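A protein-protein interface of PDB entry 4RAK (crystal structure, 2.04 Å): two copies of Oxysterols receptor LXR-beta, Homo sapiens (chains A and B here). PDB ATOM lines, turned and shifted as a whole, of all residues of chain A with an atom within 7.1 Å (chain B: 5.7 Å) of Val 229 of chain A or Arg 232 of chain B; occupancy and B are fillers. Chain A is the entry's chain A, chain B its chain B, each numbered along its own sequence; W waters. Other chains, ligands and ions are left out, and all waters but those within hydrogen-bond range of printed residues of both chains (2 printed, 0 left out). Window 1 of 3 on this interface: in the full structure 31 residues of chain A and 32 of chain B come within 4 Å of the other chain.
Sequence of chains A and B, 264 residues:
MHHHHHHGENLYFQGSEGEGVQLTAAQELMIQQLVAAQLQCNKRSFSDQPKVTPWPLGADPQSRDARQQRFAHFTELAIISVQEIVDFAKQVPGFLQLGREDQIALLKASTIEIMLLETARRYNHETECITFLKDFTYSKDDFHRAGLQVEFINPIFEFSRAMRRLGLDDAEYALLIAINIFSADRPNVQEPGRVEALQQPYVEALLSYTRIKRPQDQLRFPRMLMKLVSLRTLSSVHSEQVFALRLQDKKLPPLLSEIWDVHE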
ATOM      1  N   MET A 224     -19.928 -18.996  34.231  1.00  0.00           N
ATOM      2  CA  MET A 224     -20.133 -17.680  33.625  1.00  0.00           C
ATOM      3  C   MET A 224     -19.813 -17.752  32.132  1.00  0.00           C
ATOM      4  O   MET A 224     -20.617 -17.362  31.270  1.00  0.00           O
ATOM      5  CB  MET A 224     -19.156 -16.696  34.298  1.00  0.00           C
ATOM      6  CG  MET A 224     -19.754 -15.408  34.728  1.00  0.00           C
ATOM      7  SD  MET A 224     -18.563 -14.486  35.715  1.00  0.00           S
ATOM      8  CE  MET A 224     -18.718 -15.306  37.280  1.00  0.00           C
ATOM      9  N   LEU A 225     -18.616 -18.258  31.843  1.00  0.00           N
ATOM     10  CA  LEU A 225     -18.106 -18.462  30.478  1.00  0.00           C
ATOM     11  C   LEU A 225     -19.036 -19.329  29.670  1.00  0.00           C
ATOM     12  O   LEU A 225     -19.160 -19.119  28.460  1.00  0.00           O
ATOM     13  CB  LEU A 225     -16.732 -19.107  30.573  1.00  0.00           C
ATOM     14  CG  LEU A 225     -15.542 -18.401  29.944  1.00  0.00           C
ATOM     15  CD1 LEU A 225     -15.457 -16.923  30.344  1.00  0.00           C
ATOM     16  CD2 LEU A 225     -14.267 -19.134  30.267  1.00  0.00           C
ATOM     17  N   MET A 226     -19.688 -20.302  30.341  1.00  0.00           N
ATOM     18  CA  MET A 226     -20.619 -21.258  29.718  1.00  0.00           C
ATOM     19  C   MET A 226     -21.907 -20.574  29.269  1.00  0.00           C
ATOM     20  O   MET A 226     -22.573 -21.068  28.360  1.00  0.00           O
ATOM     21  CB  MET A 226     -20.934 -22.426  30.676  1.00  0.00           C
ATOM     22  CG  MET A 226     -20.973 -23.776  30.004  1.00  0.00           C
ATOM     23  SD  MET A 226     -19.432 -24.730  30.103  1.00  0.00           S
ATOM     24  CE  MET A 226     -18.588 -24.024  28.747  1.00  0.00           C
ATOM     25  N   LYS A 227     -22.274 -19.446  29.898  1.00  0.00           N
ATOM     26  CA  LYS A 227     -23.436 -18.664  29.494  1.00  0.00           C
ATOM     27  C   LYS A 227     -23.274 -18.030  28.105  1.00  0.00           C
ATOM     28  O   LYS A 227     -24.272 -17.677  27.493  1.00  0.00           O
ATOM     29  CB  LYS A 227     -23.849 -17.620  30.552  1.00  0.00           C
ATOM     30  CG  LYS A 227     -23.980 -18.152  31.983  1.00  0.00           C
ATOM     31  CD  LYS A 227     -24.833 -19.405  32.152  1.00  0.00           C
ATOM     32  CE  LYS A 227     -26.309 -19.116  32.287  1.00  0.00           C
ATOM     33  NZ  LYS A 227     -27.023 -20.356  32.687  1.00  0.00           N
ATOM     34  N   LEU A 228     -22.019 -17.914  27.599  1.00  0.00           N
ATOM     35  CA  LEU A 228     -21.721 -17.417  26.253  1.00  0.00           C
ATOM     36  C   LEU A 228     -22.156 -18.490  25.243  1.00  0.00           C
ATOM     37  O   LEU A 228     -22.516 -18.169  24.134  1.00  0.00           O
ATOM     38  CB  LEU A 228     -20.217 -17.132  26.105  1.00  0.00           C
ATOM     39  CG  LEU A 228     -19.672 -15.676  26.182  1.00  0.00           C
ATOM     40  CD1 LEU A 228     -20.452 -14.775  27.130  1.00  0.00           C
ATOM     41  CD2 LEU A 228     -18.214 -15.678  26.576  1.00  0.00           C
ATOM     42  N   VAL A 229     -22.103 -19.769  25.662  1.00  0.00           N
ATOM     43  CA  VAL A 229     -22.470 -20.931  24.853  1.00  0.00           C
ATOM     44  C   VAL A 229     -23.964 -20.853  24.575  1.00  0.00           C
ATOM     45  O   VAL A 229     -24.368 -20.739  23.424  1.00  0.00           O
ATOM     46  CB  VAL A 229     -22.051 -22.280  25.522  1.00  0.00           C
ATOM     47  CG1 VAL A 229     -22.469 -23.481  24.673  1.00  0.00           C
ATOM     48  CG2 VAL A 229     -20.566 -22.328  25.790  1.00  0.00           C
ATOM     49  N   SER A 230     -24.780 -20.829  25.638  1.00  0.00           N
ATOM     50  CA  SER A 230     -26.242 -20.740  25.545  1.00  0.00           C
ATOM     51  C   SER A 230     -26.675 -19.421  24.889  1.00  0.00           C
ATOM     52  O   SER A 230     -27.670 -19.364  24.162  1.00  0.00           O
ATOM     53  CB  SER A 230     -26.867 -20.946  26.935  1.00  0.00           C
ATOM     54  OG  SER A 230     -26.764 -19.788  27.718  1.00  0.00           O
ATOM     55  N   LEU A 231     -25.900 -18.367  25.116  1.00  0.00           N
ATOM     56  CA  LEU A 231     -26.121 -17.071  24.498  1.00  0.00           C
ATOM     57  C   LEU A 231     -25.939 -17.148  22.958  1.00  0.00           C
ATOM     58  O   LEU A 231     -26.729 -16.579  22.211  1.00  0.00           O
ATOM     59  CB  LEU A 231     -25.187 -16.047  25.147  1.00  0.00           C
ATOM     60  CG  LEU A 231     -25.398 -14.582  24.909  1.00  0.00           C
ATOM     61  CD1 LEU A 231     -26.724 -14.096  25.460  1.00  0.00           C
ATOM     62  CD2 LEU A 231     -24.258 -13.795  25.526  1.00  0.00           C
ATOM     63  N   ARG A 232     -24.964 -17.936  22.495  1.00  0.00           N
ATOM     64  CA  ARG A 232     -24.746 -18.141  21.056  1.00  0.00           C
ATOM     65  C   ARG A 232     -25.941 -18.845  20.370  1.00  0.00           C
ATOM     66  O   ARG A 232     -26.317 -18.469  19.278  1.00  0.00           O
ATOM     67  CB  ARG A 232     -23.429 -18.880  20.825  1.00  0.00           C
ATOM     68  CG  ARG A 232     -22.905 -18.821  19.420  1.00  0.00           C
ATOM     69  CD  ARG A 232     -22.606 -17.415  18.926  1.00  0.00           C
ATOM     70  NE  ARG A 232     -21.429 -16.796  19.535  1.00  0.00           N
ATOM     71  CZ  ARG A 232     -20.190 -16.920  19.068  1.00  0.00           C
ATOM     72  NH1 ARG A 232     -19.946 -17.679  18.026  1.00  0.00           N
ATOM     73  NH2 ARG A 232     -19.197 -16.270  19.628  1.00  0.00           N
ATOM     74  N   THR A 233     -26.569 -19.815  21.038  1.00  0.00           N
ATOM     75  CA  THR A 233     -27.782 -20.482  20.547  1.00  0.00           C
ATOM     76  C   THR A 233     -29.013 -19.541  20.568  1.00  0.00           C
ATOM     77  O   THR A 233     -29.791 -19.525  19.604  1.00  0.00           O
ATOM     78  CB  THR A 233     -27.974 -21.795  21.291  1.00  0.00           C
ATOM     79  OG1 THR A 233     -26.900 -22.651  20.904  1.00  0.00           O
ATOM     80  CG2 THR A 233     -29.289 -22.479  20.961  1.00  0.00           C
ATOM     81  N   LEU A 234     -29.165 -18.723  21.630  1.00  0.00           N
ATOM     82  CA  LEU A 234     -30.243 -17.719  21.701  1.00  0.00           C
ATOM     83  C   LEU A 234     -30.212 -16.722  20.548  1.00  0.00           C
ATOM     84  O   LEU A 234     -31.258 -16.342  20.017  1.00  0.00           O
ATOM     85  CB  LEU A 234     -30.213 -16.951  23.029  1.00  0.00           C
ATOM     86  CG  LEU A 234     -30.821 -17.603  24.257  1.00  0.00           C
ATOM     87  CD1 LEU A 234     -30.566 -16.753  25.506  1.00  0.00           C
ATOM     88  CD2 LEU A 234     -32.312 -17.755  24.110  1.00  0.00           C
ATOM     89  N   SER A 236     -28.710 -17.183  17.485  1.00  0.00           N
ATOM     90  CA  SER A 236     -28.983 -17.883  16.230  1.00  0.00           C
ATOM     91  C   SER A 236     -30.484 -18.124  16.014  1.00  0.00           C
ATOM     92  O   SER A 236     -30.969 -17.964  14.898  1.00  0.00           O
ATOM     93  CB  SER A 236     -28.193 -19.184  16.151  1.00  0.00           C
ATOM     94  OG  SER A 236     -28.560 -20.067  17.186  1.00  0.00           O
ATOM     95  N   GLU B 113     -22.032 -31.600  16.879  1.00  0.00           N
ATOM     96  CA  GLU B 113     -20.925 -30.990  17.612  1.00  0.00           C
ATOM     97  C   GLU B 113     -19.848 -31.984  18.019  1.00  0.00           C
ATOM     98  O   GLU B 113     -18.657 -31.664  17.938  1.00  0.00           O
ATOM     99  CB  GLU B 113     -21.484 -30.218  18.807  1.00  0.00           C
ATOM    100  CG  GLU B 113     -22.591 -29.234  18.465  1.00  0.00           C
ATOM    101  CD  GLU B 113     -23.021 -28.368  19.633  1.00  0.00           C
ATOM    102  OE1 GLU B 113     -24.091 -27.758  19.554  1.00  0.00           O
ATOM    103  OE2 GLU B 113     -22.274 -28.304  20.630  1.00  0.00           O
ATOM    104  N   SER B 183     -25.381 -30.661  28.201  1.00  0.00           N
ATOM    105  CA  SER B 183     -25.784 -29.268  28.033  1.00  0.00           C
ATOM    106  C   SER B 183     -27.275 -29.083  28.391  1.00  0.00           C
ATOM    107  O   SER B 183     -28.144 -29.594  27.700  1.00  0.00           O
ATOM    108  CB  SER B 183     -25.486 -28.828  26.602  1.00  0.00           C
ATOM    109  OG  SER B 183     -24.086 -28.707  26.404  1.00  0.00           O
ATOM    110  N   ASP B 185     -29.359 -26.513  28.195  1.00  0.00           N
ATOM    111  CA  ASP B 185     -30.133 -25.586  27.354  1.00  0.00           C
ATOM    112  C   ASP B 185     -30.664 -26.199  26.045  1.00  0.00           C
ATOM    113  O   ASP B 185     -31.310 -25.527  25.243  1.00  0.00           O
ATOM    114  CB  ASP B 185     -29.291 -24.348  27.057  1.00  0.00           C
ATOM    115  CG  ASP B 185     -28.153 -24.607  26.073  1.00  0.00           C
ATOM    116  OD1 ASP B 185     -27.443 -25.630  26.244  1.00  0.00           O
ATOM    117  OD2 ASP B 185     -28.010 -23.811  25.125  1.00  0.00           O
ATOM    118  N   ARG B 186     -30.379 -27.477  25.833  1.00  0.00           N
ATOM    119  CA  ARG B 186     -30.804 -28.194  24.632  1.00  0.00           C
ATOM    120  C   ARG B 186     -32.331 -28.290  24.529  1.00  0.00           C
ATOM    121  O   ARG B 186     -33.006 -28.407  25.564  1.00  0.00           O
ATOM    122  CB  ARG B 186     -30.214 -29.609  24.598  1.00  0.00           C
ATOM    123  CG  ARG B 186     -28.691 -29.719  24.593  1.00  0.00           C
ATOM    124  CD  ARG B 186     -27.981 -28.957  23.494  1.00  0.00           C
ATOM    125  NE  ARG B 186     -26.618 -29.461  23.369  1.00  0.00           N
ATOM    126  CZ  ARG B 186     -25.724 -29.009  22.513  1.00  0.00           C
ATOM    127  NH1 ARG B 186     -26.045 -28.048  21.671  1.00  0.00           N
ATOM    128  NH2 ARG B 186     -24.516 -29.516  22.502  1.00  0.00           N
ATOM    129  N   LEU B 225     -13.058 -24.192  26.721  1.00  0.00           N
ATOM    130  CA  LEU B 225     -14.479 -23.983  26.984  1.00  0.00           C
ATOM    131  C   LEU B 225     -15.075 -23.065  25.915  1.00  0.00           C
ATOM    132  O   LEU B 225     -16.230 -23.229  25.541  1.00  0.00           O
ATOM    133  CB  LEU B 225     -14.615 -23.330  28.336  1.00  0.00           C
ATOM    134  CG  LEU B 225     -15.106 -24.111  29.541  1.00  0.00           C
ATOM    135  CD1 LEU B 225     -14.838 -25.609  29.434  1.00  0.00           C
ATOM    136  CD2 LEU B 225     -14.601 -23.468  30.826  1.00  0.00           C
ATOM    137  N   LYS B 227     -14.319 -23.033  22.844  1.00  0.00           N
ATOM    138  CA  LYS B 227     -14.534 -23.840  21.654  1.00  0.00           C
ATOM    139  C   LYS B 227     -15.938 -24.419  21.651  1.00  0.00           C
ATOM    140  O   LYS B 227     -16.475 -24.712  20.596  1.00  0.00           O
ATOM    141  CB  LYS B 227     -13.461 -24.926  21.507  1.00  0.00           C
ATOM    142  CG  LYS B 227     -12.031 -24.456  21.647  1.00  0.00           C
ATOM    143  CD  LYS B 227     -11.606 -23.306  20.727  1.00  0.00           C
ATOM    144  CE  LYS B 227     -11.493 -23.654  19.261  1.00  0.00           C
ATOM    145  NZ  LYS B 227     -11.558 -22.413  18.445  1.00  0.00           N
ATOM    146  N   LEU B 228     -16.566 -24.528  22.824  1.00  0.00           N
ATOM    147  CA  LEU B 228     -17.953 -24.989  22.920  1.00  0.00           C
ATOM    148  C   LEU B 228     -18.898 -23.906  22.319  1.00  0.00           C
ATOM    149  O   LEU B 228     -20.001 -24.227  21.839  1.00  0.00           O
ATOM    150  CB  LEU B 228     -18.308 -25.248  24.398  1.00  0.00           C
ATOM    151  CG  LEU B 228     -18.245 -26.688  24.998  1.00  0.00           C
ATOM    152  CD1 LEU B 228     -17.208 -27.569  24.383  1.00  0.00           C
ATOM    153  CD2 LEU B 228     -18.056 -26.647  26.483  1.00  0.00           C
ATOM    154  N   VAL B 229     -18.476 -22.631  22.426  1.00  0.00           N
ATOM    155  CA  VAL B 229     -19.186 -21.474  21.868  1.00  0.00           C
ATOM    156  C   VAL B 229     -19.116 -21.578  20.354  1.00  0.00           C
ATOM    157  O   VAL B 229     -20.169 -21.502  19.698  1.00  0.00           O
ATOM    158  CB  VAL B 229     -18.647 -20.111  22.398  1.00  0.00           C
ATOM    159  CG1 VAL B 229     -19.466 -18.955  21.854  1.00  0.00           C
ATOM    160  CG2 VAL B 229     -18.629 -20.084  23.915  1.00  0.00           C
ATOM    161  N   SER B 230     -17.902 -21.854  19.810  1.00  0.00           N
ATOM    162  CA  SER B 230     -17.651 -22.036  18.366  1.00  0.00           C
ATOM    163  C   SER B 230     -18.483 -23.146  17.776  1.00  0.00           C
ATOM    164  O   SER B 230     -18.995 -23.033  16.650  1.00  0.00           O
ATOM    165  CB  SER B 230     -16.165 -22.313  18.099  1.00  0.00           C
ATOM    166  OG  SER B 230     -15.381 -21.188  18.442  1.00  0.00           O
ATOM    167  N   LEU B 231     -18.645 -24.228  18.551  1.00  0.00           N
ATOM    168  CA  LEU B 231     -19.431 -25.382  18.168  1.00  0.00           C
ATOM    169  C   LEU B 231     -20.901 -25.007  17.976  1.00  0.00           C
ATOM    170  O   LEU B 231     -21.548 -25.561  17.100  1.00  0.00           O
ATOM    171  CB  LEU B 231     -19.293 -26.461  19.244  1.00  0.00           C
ATOM    172  CG  LEU B 231     -18.432 -27.700  19.024  1.00  0.00           C
ATOM    173  CD1 LEU B 231     -17.793 -27.772  17.671  1.00  0.00           C
ATOM    174  CD2 LEU B 231     -17.472 -27.908  20.162  1.00  0.00           C
ATOM    175  N   ARG B 232     -21.432 -24.090  18.804  1.00  0.00           N
ATOM    176  CA  ARG B 232     -22.823 -23.656  18.654  1.00  0.00           C
ATOM    177  C   ARG B 232     -23.088 -23.042  17.278  1.00  0.00           C
ATOM    178  O   ARG B 232     -24.046 -23.408  16.613  1.00  0.00           O
ATOM    179  CB  ARG B 232     -23.268 -22.714  19.759  1.00  0.00           C
ATOM    180  CG  ARG B 232     -23.452 -23.356  21.129  1.00  0.00           C
ATOM    181  CD  ARG B 232     -24.324 -24.618  21.126  1.00  0.00           C
ATOM    182  NE  ARG B 232     -24.323 -25.253  22.450  1.00  0.00           N
ATOM    183  CZ  ARG B 232     -25.341 -25.229  23.298  1.00  0.00           C
ATOM    184  NH1 ARG B 232     -26.462 -24.596  22.984  1.00  0.00           N
ATOM    185  NH2 ARG B 232     -25.236 -25.815  24.476  1.00  0.00           N
ATOM    186  N   THR B 233     -22.206 -22.144  16.854  1.00  0.00           N
ATOM    187  CA  THR B 233     -22.228 -21.459  15.564  1.00  0.00           C
ATOM    188  C   THR B 233     -22.074 -22.470  14.428  1.00  0.00           C
ATOM    189  O   THR B 233     -22.829 -22.401  13.450  1.00  0.00           O
ATOM    190  CB  THR B 233     -21.106 -20.412  15.551  1.00  0.00           C
ATOM    191  OG1 THR B 233     -21.433 -19.399  16.494  1.00  0.00           O
ATOM    192  CG2 THR B 233     -20.910 -19.776  14.186  1.00  0.00           C
ATOM    193  N   LEU B 234     -21.121 -23.416  14.564  1.00  0.00           N
ATOM    194  CA  LEU B 234     -20.877 -24.423  13.550  1.00  0.00           C
ATOM    195  C   LEU B 234     -22.132 -25.245  13.293  1.00  0.00           C
ATOM    196  O   LEU B 234     -22.491 -25.442  12.142  1.00  0.00           O
ATOM    197  CB  LEU B 234     -19.682 -25.299  13.919  1.00  0.00           C
ATOM    198  CG  LEU B 234     -18.275 -24.749  13.649  1.00  0.00           C
ATOM    199  CD1 LEU B 234     -17.229 -25.552  14.397  1.00  0.00           C
ATOM    200  CD2 LEU B 234     -17.908 -24.845  12.180  1.00  0.00           C
ATOM    201  N   SER B 235     -22.825 -25.675  14.369  1.00  0.00           N
ATOM    202  CA  SER B 235     -24.069 -26.405  14.258  1.00  0.00           C
ATOM    203  C   SER B 235     -25.152 -25.564  13.512  1.00  0.00           C
ATOM    204  O   SER B 235     -25.919 -26.110  12.741  1.00  0.00           O
ATOM    205  CB  SER B 235     -24.573 -26.794  15.635  1.00  0.00           C
ATOM    206  OG  SER B 235     -25.904 -27.288  15.542  1.00  0.00           O
ATOM    207  N   SER B 236     -25.208 -24.258  13.789  1.00  0.00           N
ATOM    208  CA  SER B 236     -26.124 -23.303  13.172  1.00  0.00           C
ATOM    209  C   SER B 236     -25.797 -23.121  11.677  1.00  0.00           C
ATOM    210  O   SER B 236     -26.710 -23.071  10.870  1.00  0.00           O
ATOM    211  CB  SER B 236     -26.060 -21.964  13.907  1.00  0.00           C
ATOM    212  OG  SER B 236     -26.677 -20.933  13.164  1.00  0.00           O
ATOM    213  N   VAL B 237     -24.502 -23.055  11.323  1.00  0.00           N
ATOM    214  CA  VAL B 237     -24.040 -22.954   9.935  1.00  0.00           C
ATOM    215  C   VAL B 237     -24.444 -24.242   9.221  1.00  0.00           C
ATOM    216  O   VAL B 237     -25.071 -24.176   8.171  1.00  0.00           O
ATOM    217  CB  VAL B 237     -22.518 -22.639   9.842  1.00  0.00           C
ATOM    218  CG1 VAL B 237     -21.949 -22.934   8.455  1.00  0.00           C
ATOM    219  CG2 VAL B 237     -22.236 -21.206  10.249  1.00  0.00           C
HETATM  220  O   HOH W   1     -26.462 -23.054  17.667  1.00  0.00           O
HETATM  221  O   HOH W   2     -29.432 -21.541  24.424  1.00  0.00           O
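The side-chain hydroxyl of Thr 233 of chain A lies within hydrogen-bond range of the guanidinium group of Arg 232 of chain B (2.9 Å). The guanidinium group of Arg 232 of chain A is in hydrogen-bond range of the side-chain hydroxyl of Thr 233 of chain B (2.7 Å).
OE1 of Glu 113 of chain B is in salt-bridge range of NE of Arg 232 of chain B (3.8 Å). OG of Ser 236 of chain A sits at hydrogen-bond distance from O of Arg 232 of chain A, 3.5 Å away. The side-chain carboxylate (OD2) of Asp 185 of chain B lies within salt-bridge range of the guanidinium group (NH1) of Arg 232 of chain B (2.8 Å). The side-chain hydroxyl (OG) of Ser 236 of chain A sits at hydrogen-bond distance from the backbone carbonyl oxygen (O) of Thr 233 of chain A, 2.8 Å away. The backbone carbonyl oxygen of Lys 227 of chain A is in hydrogen-bond range of the side-chain hydroxyl of Ser 230 of chain A (3.3 Å).
Leu 225 of chain B touches Met 226 of chain A (CG to CE, 3.6 Å). Leu 228 of chain B touches Met 226 of chain A (CD2 to CE, 3.5 Å). CG1 of Val 229 of chain B touches O of Leu 228 of chain A, at 3.9 Å. CG1 of Val 229 of chain A touches O of Leu 228 of chain B, at 3.8 Å. Val 229 of chain B touches Val 229 of chain A. Arg 232 of chain B touches Val 229 of chain A (NE to CG1, 3.4 Å). Ser 230 of chain A touches Asp 185 of chain B (CA to OD2, 3.6 Å). Arg 232 of chain A touches Val 229 of chain B. CB of Arg 232 of chain B touches CG of Arg 232 of chain A, at 3.9 Å. Ser 236 of chain B touches Ser 236 of chain A (OG to CB, 3.8 Å).
Of the printed residues of chain B, Arg 232 of chain A touches Val 229 (3.5 Å), Arg 232 (3.9 Å) and Thr 233 (2.7 Å). Ser 230 of chain B touches none of the printed residues of chain A. Arg 232 of chain B touches just these residues of chain A: Val 229, Arg 232 and Thr 233. Printed residues of chain A within 4 Å of Ser 236 of chain B: Ser 236. The nearest residue of chain A that does not touch Arg 232 of chain B is Ser 230 of chain A (4.6 Å). The nearest printed residue of chain B that does not touch Ser 236 of chain A is Arg 232 of chain B (5.6 Å).
Printed residues of chain A that touch a printed residue of chain B: Met 226, Leu 228, Val 229, Ser 230, Arg 232, Thr 233 and Ser 236. Hydrophobic or aromatic side chains of chain A within 4 Å of the printed part of chain B: Met 226 and Val 229. Hydrophobic or aromatic side chains of chain B that line the printed part of chain A: Leu 225, Leu 228 and Val 229.
Leu 228 of chain A touches Val 229 of chain B, and with the chains exchanged Val 229 of chain A touches Leu 228 of chain B. Val 229 of chain B touches its own counterpart, Val 229 of chain A. Arg 232 of chain A touches Thr 233 of chain B, and with the chains exchanged Thr 233 of chain A touches Arg 232 of chain B. Ser 236 of chain A touches its own counterpart, Ser 236 of chain B. Positions printed for both chains: 225, 227, 228, 229, 230, 231, 232, 233, 234 and 236. Of the 12 pairs that touch across the chains among the printed residues, 9 have their exchanged pair printed and touching as well.
Water W1 lies within hydrogen-bond range of O of Arg 232 of chain B (2.7 Å) and OG1 of Thr 233 of chain A (3.3 Å). Water W2 lies within hydrogen-bond range of the side-chain carboxylate (OD2) of Asp 185 of chain B and the backbone carbonyl oxygen (O) of Ser 230 of chain A.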
